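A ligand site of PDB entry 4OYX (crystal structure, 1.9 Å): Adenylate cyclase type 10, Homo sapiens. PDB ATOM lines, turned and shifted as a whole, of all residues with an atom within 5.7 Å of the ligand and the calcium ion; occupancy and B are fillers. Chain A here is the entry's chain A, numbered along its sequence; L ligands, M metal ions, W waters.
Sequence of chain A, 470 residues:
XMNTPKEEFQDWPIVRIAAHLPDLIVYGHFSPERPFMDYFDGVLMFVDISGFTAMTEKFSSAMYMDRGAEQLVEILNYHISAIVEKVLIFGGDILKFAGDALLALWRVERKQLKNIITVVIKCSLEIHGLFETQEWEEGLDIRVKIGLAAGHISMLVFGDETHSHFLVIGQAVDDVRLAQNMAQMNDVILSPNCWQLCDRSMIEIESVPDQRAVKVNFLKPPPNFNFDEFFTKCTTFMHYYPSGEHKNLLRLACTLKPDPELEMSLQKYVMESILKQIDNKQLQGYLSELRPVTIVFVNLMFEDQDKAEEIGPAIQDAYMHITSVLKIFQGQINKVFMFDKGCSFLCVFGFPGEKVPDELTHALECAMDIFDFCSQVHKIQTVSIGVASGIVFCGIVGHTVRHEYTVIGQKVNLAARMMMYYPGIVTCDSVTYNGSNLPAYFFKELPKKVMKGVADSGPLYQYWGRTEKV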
ATOM      1  N   ASP A  48      17.818   6.163 -39.588  1.00  0.00           N
ATOM      2  CA  ASP A  48      17.099   6.315 -38.320  1.00  0.00           C
ATOM      3  C   ASP A  48      15.625   6.167 -38.558  1.00  0.00           C
ATOM      4  O   ASP A  48      15.107   6.831 -39.456  1.00  0.00           O
ATOM      5  CB  ASP A  48      17.402   7.688 -37.706  1.00  0.00           C
ATOM      6  CG  ASP A  48      16.667   7.954 -36.415  1.00  0.00           C
ATOM      7  OD1 ASP A  48      16.999   7.297 -35.393  1.00  0.00           O
ATOM      8  OD2 ASP A  48      15.753   8.816 -36.411  1.00  0.00           O
ATOM      9  N   ILE A  49      14.932   5.288 -37.788  1.00  0.00           N
ATOM     10  CA  ILE A  49      13.464   5.349 -37.728  1.00  0.00           C
ATOM     11  C   ILE A  49      13.035   6.243 -36.561  1.00  0.00           C
ATOM     12  O   ILE A  49      13.500   6.078 -35.415  1.00  0.00           O
ATOM     13  CB  ILE A  49      12.653   3.999 -37.752  1.00  0.00           C
ATOM     14  CG1 ILE A  49      13.334   2.825 -38.578  1.00  0.00           C
ATOM     15  CG2 ILE A  49      11.186   4.231 -38.235  1.00  0.00           C
ATOM     16  CD1 ILE A  49      13.914   3.106 -39.875  1.00  0.00           C
ATOM     17  N   SER A  50      12.133   7.192 -36.854  1.00  0.00           N
ATOM     18  CA  SER A  50      11.533   8.058 -35.835  1.00  0.00           C
ATOM     19  C   SER A  50      10.067   7.699 -35.680  1.00  0.00           C
ATOM     20  O   SER A  50       9.383   7.492 -36.678  1.00  0.00           O
ATOM     21  CB  SER A  50      11.681   9.541 -36.204  1.00  0.00           C
ATOM     22  OG  SER A  50      11.110  10.397 -35.225  1.00  0.00           O
ATOM     23  N   GLY A  51       9.616   7.639 -34.429  1.00  0.00           N
ATOM     24  CA  GLY A  51       8.230   7.353 -34.057  1.00  0.00           C
ATOM     25  C   GLY A  51       8.066   6.142 -33.147  1.00  0.00           C
ATOM     26  O   GLY A  51       7.015   5.991 -32.506  1.00  0.00           O
ATOM     27  N   PHE A  52       9.092   5.293 -33.066  1.00  0.00           N
ATOM     28  CA  PHE A  52       8.850   3.953 -32.575  1.00  0.00           C
ATOM     29  C   PHE A  52       8.876   3.826 -31.066  1.00  0.00           C
ATOM     30  O   PHE A  52       8.340   2.841 -30.564  1.00  0.00           O
ATOM     31  CB  PHE A  52       9.742   2.899 -33.268  1.00  0.00           C
ATOM     32  CG  PHE A  52       8.936   2.033 -34.205  1.00  0.00           C
ATOM     33  CD1 PHE A  52       8.933   2.274 -35.578  1.00  0.00           C
ATOM     34  CD2 PHE A  52       8.157   0.990 -33.716  1.00  0.00           C
ATOM     35  CE1 PHE A  52       8.174   1.471 -36.451  1.00  0.00           C
ATOM     36  CE2 PHE A  52       7.397   0.187 -34.579  1.00  0.00           C
ATOM     37  CZ  PHE A  52       7.408   0.432 -35.941  1.00  0.00           C
ATOM     38  N   THR A  53       9.474   4.803 -30.324  1.00  0.00           N
ATOM     39  CA  THR A  53       9.418   4.789 -28.844  1.00  0.00           C
ATOM     40  C   THR A  53       8.081   5.356 -28.318  1.00  0.00           C
ATOM     41  O   THR A  53       7.657   4.997 -27.208  1.00  0.00           O
ATOM     42  CB  THR A  53      10.643   5.446 -28.177  1.00  0.00           C
ATOM     43  OG1 THR A  53      10.594   6.862 -28.367  1.00  0.00           O
ATOM     44  CG2 THR A  53      11.980   4.854 -28.664  1.00  0.00           C
ATOM     45  N   ALA A  54       7.420   6.251 -29.124  1.00  0.00           N
ATOM     46  CA  ALA A  54       6.037   6.670 -28.886  1.00  0.00           C
ATOM     47  C   ALA A  54       5.121   5.489 -29.189  1.00  0.00           C
ATOM     48  O   ALA A  54       4.129   5.276 -28.477  1.00  0.00           O
ATOM     49  CB  ALA A  54       5.682   7.841 -29.769  1.00  0.00           C
ATOM     50  N   PHE A  97      22.291  -2.842 -35.478  1.00  0.00           N
ATOM     51  CA  PHE A  97      20.968  -2.279 -35.162  1.00  0.00           C
ATOM     52  C   PHE A  97      21.083  -1.553 -33.808  1.00  0.00           C
ATOM     53  O   PHE A  97      21.551  -2.125 -32.828  1.00  0.00           O
ATOM     54  CB  PHE A  97      19.860  -3.355 -35.088  1.00  0.00           C
ATOM     55  CG  PHE A  97      19.580  -4.056 -36.388  1.00  0.00           C
ATOM     56  CD1 PHE A  97      20.319  -5.170 -36.779  1.00  0.00           C
ATOM     57  CD2 PHE A  97      18.614  -3.571 -37.262  1.00  0.00           C
ATOM     58  CE1 PHE A  97      20.090  -5.800 -37.994  1.00  0.00           C
ATOM     59  CE2 PHE A  97      18.371  -4.207 -38.467  1.00  0.00           C
ATOM     60  CZ  PHE A  97      19.113  -5.312 -38.828  1.00  0.00           C
ATOM     61  N   ALA A  98      20.664  -0.297 -33.759  1.00  0.00           N
ATOM     62  CA  ALA A  98      20.562   0.474 -32.523  1.00  0.00           C
ATOM     63  C   ALA A  98      19.083   0.894 -32.369  1.00  0.00           C
ATOM     64  O   ALA A  98      18.671   1.928 -32.889  1.00  0.00           O
ATOM     65  CB  ALA A  98      21.482   1.695 -32.579  1.00  0.00           C
ATOM     66  N   GLY A  99      18.319   0.073 -31.670  1.00  0.00           N
ATOM     67  CA  GLY A  99      16.879   0.204 -31.535  1.00  0.00           C
ATOM     68  C   GLY A  99      16.151   0.078 -32.863  1.00  0.00           C
ATOM     69  O   GLY A  99      16.127  -1.000 -33.475  1.00  0.00           O
ATOM     70  N   ASP A 100      15.566   1.194 -33.317  1.00  0.00           N
ATOM     71  CA  ASP A 100      14.884   1.405 -34.599  1.00  0.00           C
ATOM     72  C   ASP A 100      15.805   2.166 -35.594  1.00  0.00           C
ATOM     73  O   ASP A 100      15.332   2.675 -36.607  1.00  0.00           O
ATOM     74  CB  ASP A 100      13.541   2.144 -34.358  1.00  0.00           C
ATOM     75  CG  ASP A 100      13.593   3.380 -33.459  1.00  0.00           C
ATOM     76  OD1 ASP A 100      12.529   3.751 -32.888  1.00  0.00           O
ATOM     77  OD2 ASP A 100      14.696   4.000 -33.339  1.00  0.00           O
ATOM     78  N   ALA A 101      17.124   2.236 -35.296  1.00  0.00           N
ATOM     79  CA  ALA A 101      18.174   2.802 -36.152  1.00  0.00           C
ATOM     80  C   ALA A 101      19.162   1.682 -36.593  1.00  0.00           C
ATOM     81  O   ALA A 101      19.247   0.629 -35.957  1.00  0.00           O
ATOM     82  CB  ALA A 101      18.904   3.907 -35.409  1.00  0.00           C
ATOM     83  N   LYS A 145      15.013   9.137 -41.608  1.00  0.00           N
ATOM     84  CA  LYS A 145      16.098  10.094 -41.918  1.00  0.00           C
ATOM     85  C   LYS A 145      17.363   9.318 -42.244  1.00  0.00           C
ATOM     86  O   LYS A 145      17.709   8.398 -41.502  1.00  0.00           O
ATOM     87  CB  LYS A 145      16.384  11.029 -40.739  1.00  0.00           C
ATOM     88  CG  LYS A 145      15.225  11.905 -40.294  1.00  0.00           C
ATOM     89  CD  LYS A 145      15.407  12.290 -38.820  1.00  0.00           C
ATOM     90  CE  LYS A 145      14.316  13.201 -38.321  1.00  0.00           C
ATOM     91  NZ  LYS A 145      14.415  13.393 -36.848  1.00  0.00           N
ATOM     92  N   ARG A 177      26.788  10.287 -38.427  1.00  0.00           N
ATOM     93  CA  ARG A 177      25.902  10.672 -37.328  1.00  0.00           C
ATOM     94  C   ARG A 177      25.518  12.174 -37.458  1.00  0.00           C
ATOM     95  O   ARG A 177      24.344  12.511 -37.385  1.00  0.00           O
ATOM     96  CB  ARG A 177      26.577  10.373 -35.979  1.00  0.00           C
ATOM     97  CG  ARG A 177      25.690  10.565 -34.727  1.00  0.00           C
ATOM     98  CD  ARG A 177      24.841   9.351 -34.347  1.00  0.00           C
ATOM     99  NE  ARG A 177      25.654   8.176 -33.996  1.00  0.00           N
ATOM    100  CZ  ARG A 177      25.227   7.183 -33.219  1.00  0.00           C
ATOM    101  NH1 ARG A 177      24.011   7.197 -32.699  1.00  0.00           N
ATOM    102  NH2 ARG A 177      26.031   6.158 -32.953  1.00  0.00           N
ATOM    103  N   PHE A 297      23.837   3.459 -19.314  1.00  0.00           N
ATOM    104  CA  PHE A 297      24.476   3.854 -20.574  1.00  0.00           C
ATOM    105  C   PHE A 297      25.764   4.535 -20.245  1.00  0.00           C
ATOM    106  O   PHE A 297      25.753   5.654 -19.703  1.00  0.00           O
ATOM    107  CB  PHE A 297      23.560   4.814 -21.358  1.00  0.00           C
ATOM    108  CG  PHE A 297      23.350   4.516 -22.821  1.00  0.00           C
ATOM    109  CD1 PHE A 297      24.428   4.462 -23.709  1.00  0.00           C
ATOM    110  CD2 PHE A 297      22.062   4.303 -23.333  1.00  0.00           C
ATOM    111  CE1 PHE A 297      24.230   4.175 -25.060  1.00  0.00           C
ATOM    112  CE2 PHE A 297      21.863   4.038 -24.684  1.00  0.00           C
ATOM    113  CZ  PHE A 297      22.944   3.969 -25.542  1.00  0.00           C
ATOM    114  N   ASN A 334      24.462  -4.869 -23.954  1.00  0.00           N
ATOM    115  CA  ASN A 334      23.640  -5.027 -25.146  1.00  0.00           C
ATOM    116  C   ASN A 334      24.380  -4.577 -26.430  1.00  0.00           C
ATOM    117  O   ASN A 334      24.411  -5.345 -27.369  1.00  0.00           O
ATOM    118  CB  ASN A 334      22.272  -4.350 -24.978  1.00  0.00           C
ATOM    119  CG  ASN A 334      21.368  -4.473 -26.182  1.00  0.00           C
ATOM    120  OD1 ASN A 334      20.838  -5.546 -26.515  1.00  0.00           O
ATOM    121  ND2 ASN A 334      21.241  -3.397 -26.919  1.00  0.00           N
ATOM    122  N   LYS A 335      24.950  -3.359 -26.471  1.00  0.00           N
ATOM    123  CA  LYS A 335      25.704  -2.868 -27.623  1.00  0.00           C
ATOM    124  C   LYS A 335      26.782  -1.930 -27.152  1.00  0.00           C
ATOM    125  O   LYS A 335      26.684  -1.359 -26.054  1.00  0.00           O
ATOM    126  CB  LYS A 335      24.825  -2.086 -28.633  1.00  0.00           C
ATOM    127  CG  LYS A 335      23.584  -2.798 -29.162  1.00  0.00           C
ATOM    128  CD  LYS A 335      23.709  -3.351 -30.569  1.00  0.00           C
ATOM    129  CE  LYS A 335      22.495  -4.187 -30.862  1.00  0.00           C
ATOM    130  NZ  LYS A 335      22.877  -5.573 -31.228  1.00  0.00           N
ATOM    131  N   PHE A 337      28.955   1.311 -29.325  1.00  0.00           N
ATOM    132  CA  PHE A 337      28.923   2.123 -30.558  1.00  0.00           C
ATOM    133  C   PHE A 337      29.438   3.557 -30.343  1.00  0.00           C
ATOM    134  O   PHE A 337      29.342   4.082 -29.235  1.00  0.00           O
ATOM    135  CB  PHE A 337      27.512   2.121 -31.178  1.00  0.00           C
ATOM    136  CG  PHE A 337      26.497   2.679 -30.228  1.00  0.00           C
ATOM    137  CD1 PHE A 337      26.255   4.043 -30.158  1.00  0.00           C
ATOM    138  CD2 PHE A 337      25.794   1.833 -29.368  1.00  0.00           C
ATOM    139  CE1 PHE A 337      25.339   4.550 -29.246  1.00  0.00           C
ATOM    140  CE2 PHE A 337      24.882   2.349 -28.466  1.00  0.00           C
ATOM    141  CZ  PHE A 337      24.660   3.706 -28.414  1.00  0.00           C
ATOM    142  N   PHE A 339      29.020   7.387 -30.729  1.00  0.00           N
ATOM    143  CA  PHE A 339      27.814   8.225 -30.778  1.00  0.00           C
ATOM    144  C   PHE A 339      28.131   9.685 -30.480  1.00  0.00           C
ATOM    145  O   PHE A 339      28.351  10.038 -29.316  1.00  0.00           O
ATOM    146  CB  PHE A 339      26.708   7.636 -29.855  1.00  0.00           C
ATOM    147  CG  PHE A 339      25.628   8.573 -29.355  1.00  0.00           C
ATOM    148  CD1 PHE A 339      24.818   9.266 -30.254  1.00  0.00           C
ATOM    149  CD2 PHE A 339      25.419   8.751 -27.995  1.00  0.00           C
ATOM    150  CE1 PHE A 339      23.824  10.147 -29.793  1.00  0.00           C
ATOM    151  CE2 PHE A 339      24.409   9.618 -27.534  1.00  0.00           C
ATOM    152  CZ  PHE A 339      23.630  10.308 -28.443  1.00  0.00           C
ATOM    153  N   LEU A 346      25.864   0.368 -24.111  1.00  0.00           N
ATOM    154  CA  LEU A 346      24.469   0.214 -23.695  1.00  0.00           C
ATOM    155  C   LEU A 346      24.358  -1.051 -22.815  1.00  0.00           C
ATOM    156  O   LEU A 346      24.372  -2.184 -23.317  1.00  0.00           O
ATOM    157  CB  LEU A 346      23.551   0.132 -24.928  1.00  0.00           C
ATOM    158  CG  LEU A 346      22.030   0.459 -24.729  1.00  0.00           C
ATOM    159  CD1 LEU A 346      21.286   0.348 -26.007  1.00  0.00           C
ATOM    160  CD2 LEU A 346      21.373  -0.448 -23.719  1.00  0.00           C
ATOM    161  N   THR A 406      17.756  -6.162 -29.652  1.00  0.00           N
ATOM    162  CA  THR A 406      17.743  -4.711 -29.378  1.00  0.00           C
ATOM    163  C   THR A 406      16.849  -4.338 -28.190  1.00  0.00           C
ATOM    164  O   THR A 406      15.943  -5.079 -27.855  1.00  0.00           O
ATOM    165  CB  THR A 406      17.343  -3.870 -30.636  1.00  0.00           C
ATOM    166  OG1 THR A 406      17.707  -4.538 -31.827  1.00  0.00           O
ATOM    167  CG2 THR A 406      18.133  -2.648 -30.697  1.00  0.00           C
ATOM    168  N   VAL A 407      17.121  -3.214 -27.566  1.00  0.00           N
ATOM    169  CA  VAL A 407      16.210  -2.615 -26.580  1.00  0.00           C
ATOM    170  C   VAL A 407      15.672  -1.325 -27.206  1.00  0.00           C
ATOM    171  O   VAL A 407      16.471  -0.568 -27.785  1.00  0.00           O
ATOM    172  CB  VAL A 407      16.921  -2.352 -25.239  1.00  0.00           C
ATOM    173  CG1 VAL A 407      17.158  -3.651 -24.486  1.00  0.00           C
ATOM    174  CG2 VAL A 407      18.243  -1.622 -25.457  1.00  0.00           C
ATOM    175  N   ILE A 408      14.343  -1.065 -27.102  1.00  0.00           N
ATOM    176  CA  ILE A 408      13.692   0.148 -27.615  1.00  0.00           C
ATOM    177  C   ILE A 408      12.774   0.712 -26.531  1.00  0.00           C
ATOM    178  O   ILE A 408      11.997  -0.044 -25.931  1.00  0.00           O
ATOM    179  CB  ILE A 408      12.880  -0.172 -28.923  1.00  0.00           C
ATOM    180  CG1 ILE A 408      13.778  -0.759 -30.019  1.00  0.00           C
ATOM    181  CG2 ILE A 408      12.055   1.040 -29.444  1.00  0.00           C
ATOM    182  CD1 ILE A 408      13.070  -1.213 -31.277  1.00  0.00           C
ATOM    183  N   GLY A 409      12.865   2.022 -26.298  1.00  0.00           N
ATOM    184  CA  GLY A 409      11.889   2.689 -25.453  1.00  0.00           C
ATOM    185  C   GLY A 409      12.349   4.059 -25.022  1.00  0.00           C
ATOM    186  O   GLY A 409      13.532   4.373 -25.111  1.00  0.00           O
ATOM    187  N   GLN A 410      11.421   4.867 -24.540  1.00  0.00           N
ATOM    188  CA  GLN A 410      11.707   6.196 -23.988  1.00  0.00           C
ATOM    189  C   GLN A 410      12.784   6.131 -22.904  1.00  0.00           C
ATOM    190  O   GLN A 410      13.592   7.023 -22.847  1.00  0.00           O
ATOM    191  CB  GLN A 410      10.420   6.829 -23.458  1.00  0.00           C
ATOM    192  CG  GLN A 410       9.412   7.128 -24.571  1.00  0.00           C
ATOM    193  CD  GLN A 410       9.509   8.504 -25.187  1.00  0.00           C
ATOM    194  OE1 GLN A 410      10.583   9.001 -25.574  1.00  0.00           O
ATOM    195  NE2 GLN A 410       8.347   9.132 -25.352  1.00  0.00           N
ATOM    196  N   VAL A 412      15.440   4.042 -22.720  1.00  0.00           N
ATOM    197  CA  VAL A 412      16.725   3.921 -23.441  1.00  0.00           C
ATOM    198  C   VAL A 412      17.151   5.305 -23.983  1.00  0.00           C
ATOM    199  O   VAL A 412      18.299   5.705 -23.790  1.00  0.00           O
ATOM    200  CB  VAL A 412      16.666   2.832 -24.556  1.00  0.00           C
ATOM    201  CG1 VAL A 412      18.062   2.500 -25.081  1.00  0.00           C
ATOM    202  CG2 VAL A 412      15.994   1.556 -24.061  1.00  0.00           C
ATOM    203  N   ASN A 413      16.228   6.055 -24.645  1.00  0.00           N
ATOM    204  CA  ASN A 413      16.535   7.420 -25.122  1.00  0.00           C
ATOM    205  C   ASN A 413      16.991   8.294 -23.979  1.00  0.00           C
ATOM    206  O   ASN A 413      17.950   9.045 -24.111  1.00  0.00           O
ATOM    207  CB  ASN A 413      15.284   8.092 -25.771  1.00  0.00           C
ATOM    208  CG  ASN A 413      14.749   7.362 -26.952  1.00  0.00           C
ATOM    209  OD1 ASN A 413      15.124   6.216 -27.259  1.00  0.00           O
ATOM    210  ND2 ASN A 413      13.865   8.022 -27.666  1.00  0.00           N
ATOM    211  N   LEU A 414      16.284   8.187 -22.851  1.00  0.00           N
ATOM    212  CA  LEU A 414      16.483   8.973 -21.661  1.00  0.00           C
ATOM    213  C   LEU A 414      17.872   8.768 -21.060  1.00  0.00           C
ATOM    214  O   LEU A 414      18.568   9.765 -20.843  1.00  0.00           O
ATOM    215  CB  LEU A 414      15.325   8.697 -20.659  1.00  0.00           C
ATOM    216  CG  LEU A 414      15.015   9.715 -19.522  1.00  0.00           C
ATOM    217  CD1 LEU A 414      15.158   9.142 -18.155  1.00  0.00           C
ATOM    218  CD2 LEU A 414      15.629  11.075 -19.726  1.00  0.00           C
ATOM    219  N   ALA A 416      20.585   7.567 -22.603  1.00  0.00           N
ATOM    220  CA  ALA A 416      21.510   8.056 -23.648  1.00  0.00           C
ATOM    221  C   ALA A 416      21.654   9.582 -23.595  1.00  0.00           C
ATOM    222  O   ALA A 416      22.798  10.090 -23.548  1.00  0.00           O
ATOM    223  CB  ALA A 416      21.027   7.610 -25.037  1.00  0.00           C
ATOM    224  N   ARG A 417      20.514  10.323 -23.595  1.00  0.00           N
ATOM    225  CA  ARG A 417      20.483  11.794 -23.542  1.00  0.00           C
ATOM    226  C   ARG A 417      21.012  12.367 -22.246  1.00  0.00           C
ATOM    227  O   ARG A 417      21.589  13.450 -22.272  1.00  0.00           O
ATOM    228  CB  ARG A 417      19.070  12.364 -23.850  1.00  0.00           C
ATOM    229  CG  ARG A 417      18.527  12.031 -25.248  1.00  0.00           C
ATOM    230  CD  ARG A 417      19.472  12.438 -26.365  1.00  0.00           C
ATOM    231  NE  ARG A 417      18.900  12.268 -27.707  1.00  0.00           N
ATOM    232  CZ  ARG A 417      19.496  12.673 -28.819  1.00  0.00           C
ATOM    233  NH1 ARG A 417      20.675  13.264 -28.767  1.00  0.00           N
ATOM    234  NH2 ARG A 417      18.916  12.496 -29.992  1.00  0.00           N
ATOM    235  N   LYS A 452      16.493  16.315 -26.396  1.00  0.00           N
ATOM    236  CA  LYS A 452      16.060  15.810 -27.705  1.00  0.00           C
ATOM    237  C   LYS A 452      15.668  14.351 -27.635  1.00  0.00           C
ATOM    238  O   LYS A 452      16.451  13.519 -27.153  1.00  0.00           O
ATOM    239  CB  LYS A 452      17.136  16.018 -28.794  1.00  0.00           C
ATOM    240  CG  LYS A 452      17.558  17.486 -29.052  1.00  0.00           C
ATOM    241  CD  LYS A 452      16.587  18.312 -29.943  1.00  0.00           C
ATOM    242  CE  LYS A 452      16.880  18.246 -31.426  1.00  0.00           C
ATOM    243  NZ  LYS A 452      18.159  18.916 -31.798  1.00  0.00           N
ATOM    244  N   GLY A 453      14.450  14.050 -28.108  1.00  0.00           N
ATOM    245  CA  GLY A 453      13.929  12.686 -28.161  1.00  0.00           C
ATOM    246  C   GLY A 453      13.495  12.166 -26.806  1.00  0.00           C
ATOM    247  O   GLY A 453      13.553  10.951 -26.569  1.00  0.00           O
HETATM  248  P1  LIG L   1      12.413   7.354 -31.508  1.00  0.00           P
HETATM  249  O1  LIG L   1      12.413   7.819 -30.058  1.00  0.00           O
HETATM  250  O2  LIG L   1      10.989   7.031 -31.940  1.00  0.00           O
HETATM  251  O3  LIG L   1      13.400   6.267 -31.747  1.00  0.00           O
HETATM  252  P2  LIG L   1      14.050   9.514 -32.650  1.00  0.00           P
HETATM  253  O4  LIG L   1      13.415  10.875 -33.007  1.00  0.00           O
HETATM  254  O5  LIG L   1      14.974   8.968 -33.694  1.00  0.00           O
HETATM  255  O6  LIG L   1      12.777   8.651 -32.365  1.00  0.00           O
HETATM  256  P3  LIG L   1      16.477  10.358 -30.704  1.00  0.00           P
HETATM  257  O7  LIG L   1      16.257  11.876 -30.617  1.00  0.00           O
HETATM  258  O8  LIG L   1      17.488   9.914 -31.720  1.00  0.00           O
HETATM  259  C1  LIG L   1      14.851   9.626 -31.030  1.00  0.00           C
HETATM  260  O9  LIG L   1      16.818   9.976 -29.202  1.00  0.00           O
HETATM  261  C2  LIG L   1      17.188   8.632 -28.866  1.00  0.00           C
HETATM  262  C3  LIG L   1      18.623   8.631 -28.375  1.00  0.00           C
HETATM  263  O10 LIG L   1      18.858   7.453 -27.607  1.00  0.00           O
HETATM  264  C4  LIG L   1      19.693   8.646 -29.471  1.00  0.00           C
HETATM  265  O11 LIG L   1      20.734   9.540 -29.094  1.00  0.00           O
HETATM  266  C5  LIG L   1      20.162   7.175 -29.576  1.00  0.00           C
HETATM  267  O12 LIG L   1      21.565   7.084 -29.771  1.00  0.00           O
HETATM  268  C6  LIG L   1      19.829   6.588 -28.190  1.00  0.00           C
HETATM  269  N1  LIG L   1      19.289   5.232 -28.243  1.00  0.00           N
HETATM  270  C7  LIG L   1      17.983   4.844 -28.022  1.00  0.00           C
HETATM  271  N2  LIG L   1      17.819   3.547 -28.137  1.00  0.00           N
HETATM  272  C8  LIG L   1      19.080   3.043 -28.433  1.00  0.00           C
HETATM  273  C9  LIG L   1      19.598   1.755 -28.669  1.00  0.00           C
HETATM  274  N3  LIG L   1      18.860   0.652 -28.621  1.00  0.00           N
HETATM  275  N4  LIG L   1      20.914   1.608 -28.950  1.00  0.00           N
HETATM  276  C10 LIG L   1      21.678   2.720 -28.977  1.00  0.00           C
HETATM  277  N5  LIG L   1      21.298   3.972 -28.776  1.00  0.00           N
HETATM  278  C11 LIG L   1      19.988   4.085 -28.506  1.00  0.00           C
HETATM  279 CA    CA M   1      15.921   5.911 -34.068  1.00  0.00          CA
HETATM  280  O   HOH W   1       8.877   8.378 -31.017  1.00  0.00           O
HETATM  281  O   HOH W   2      14.934   3.571 -27.826  1.00  0.00           O
HETATM  282  O   HOH W   3      11.864  10.379 -29.325  1.00  0.00           O
HETATM  283  O   HOH W   4      13.512  13.446 -31.365  1.00  0.00           O
HETATM  284  O   HOH W   5      21.581   5.398 -31.926  1.00  0.00           O
HETATM  285  O   HOH W   6      23.192   0.155 -30.050  1.00  0.00           O
HETATM  286  O   HOH W   7      15.766   3.324 -30.815  1.00  0.00           O
HETATM  287  O   HOH W   8      16.645   6.178 -31.514  1.00  0.00           O
HETATM  288  O   HOH W   9      20.371  -1.946 -28.855  1.00  0.00           O
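The calcium ion is bound by the side-chain carboxylate (OD1) of Asp 48 (2.2 Å), the side-chain carboxylate (OD2) of Asp 100 (2.4 Å), water W8 (2.7 Å) and the backbone carbonyl oxygen (O) of Ile 49 (2.8 Å).
The side-chain carboxylate (OD2) of Asp 48 sits close to an oxygen (O5) of the ligand (2.8 Å).
OD2 of Asp 100 sits close to O3 of the ligand, at 3.1 Å.
The backbone NH (N) of Thr 53 sits at hydrogen-bond distance from an oxygen (O2) of the ligand.
The side-chain hydroxyl (OG1) of Thr 53 is in hydrogen-bond range of an oxygen (O1) of the ligand (2.7 Å).
NH2 of Arg 417 lies within salt-bridge range of O7 of the ligand, at 2.8 Å.
The side-chain amide nitrogen (ND2) of Asn 413 is in hydrogen-bond range of an oxygen (O1) of the ligand, 2.8 Å away.
The backbone NH of Phe 52 lies within hydrogen-bond range of an oxygen (O2) of the ligand.
The backbone carbonyl oxygen of Val 407 sits at hydrogen-bond distance from a nitrogen (N3) of the ligand.
N of Gly 51 sits at hydrogen-bond distance from O2 of the ligand.
The side-chain hydroxyl of Ser 50 is in hydrogen-bond range of an oxygen (O4) of the ligand (3.2 Å).
The backbone NH (N) of Asp 48 lies within hydrogen-bond range of the backbone carbonyl oxygen (O) of Lys 145.
O of Lys 452 is in hydrogen-bond range of NE of Arg 417 (2.8 Å).
The backbone carbonyl oxygen (O) of Gly 453 is in hydrogen-bond range of the side-chain amide nitrogen (ND2) of Asn 413.
The backbone carbonyl oxygen (O) of Gly 409 sits close to the side-chain amide oxygen (OD1) of Asn 413, 3.2 Å away.
The backbone carbonyl oxygen (O) of Leu 346 is in hydrogen-bond range of the backbone NH (N) of Asn 334 (2.8 Å).
The backbone NH of Leu 346 lies within hydrogen-bond range of the backbone carbonyl oxygen of Lys 335 (2.7 Å).
Residues that only touch the calcium ion: Ala 101.
Within 4 Å of the calcium ion: Asp 48, Ile 49, Asp 100 and Ala 101.
A nitrogen (N3) of the ligand lies close to the backbone NH of Gly 99 (3.2 Å).
Residues that only touch the ligand: Phe 339, Phe 337, Leu 346, Val 412, Ala 416, Gly 453, Phe 297, Ala 98, Arg 177, Lys 452 and Thr 406.
Hydrophobic or aromatic side chains within 4 Å of the ligand: Ala 98, Phe 297, Phe 337, Phe 339, Leu 346, Val 407, Val 412 and Ala 416.
Within 4 Å of the ligand: Asp 48, Ile 49, Ser 50, Gly 51, Phe 52, Thr 53, Ala 98, Gly 99, Asp 100, Arg 177, Phe 297, Phe 337, Phe 339, Leu 346, Thr 406, Val 407, Val 412, Asn 413, Ala 416, Arg 417, Lys 452 and Gly 453.
Along chain A the residues within 4 Å of the ligand span positions 48 to 453.
The nearest printed residue that does not touch the ligand is Ala 54 (4.6 Å).
Water W1 lies within hydrogen-bond range of an oxygen (O2) of the ligand (2.7 Å), the backbone NH (N) of Ala 54 (3.2 Å) and the backbone carbonyl oxygen (O) of Gly 51 (3.4 Å).
Water W3 lies within hydrogen-bond range of O1 of the ligand (2.7 Å) and O of Gly 453 (3.3 Å).
Water W5 bridges an oxygen (O12) of the ligand (2.7 Å) and the guanidinium group (NH1) of Arg 177 (3.1 Å).
Water W9 bridges ND2 of Asn 334 (2.6 Å) and N3 of the ligand (3.0 Å).
Water W4 bridges an oxygen (O4) of the ligand and the backbone NH of Gly 453.
Water W7 bridges the backbone NH of Asp 100 (3.3 Å) and a nitrogen (N2) of the ligand (3.4 Å).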
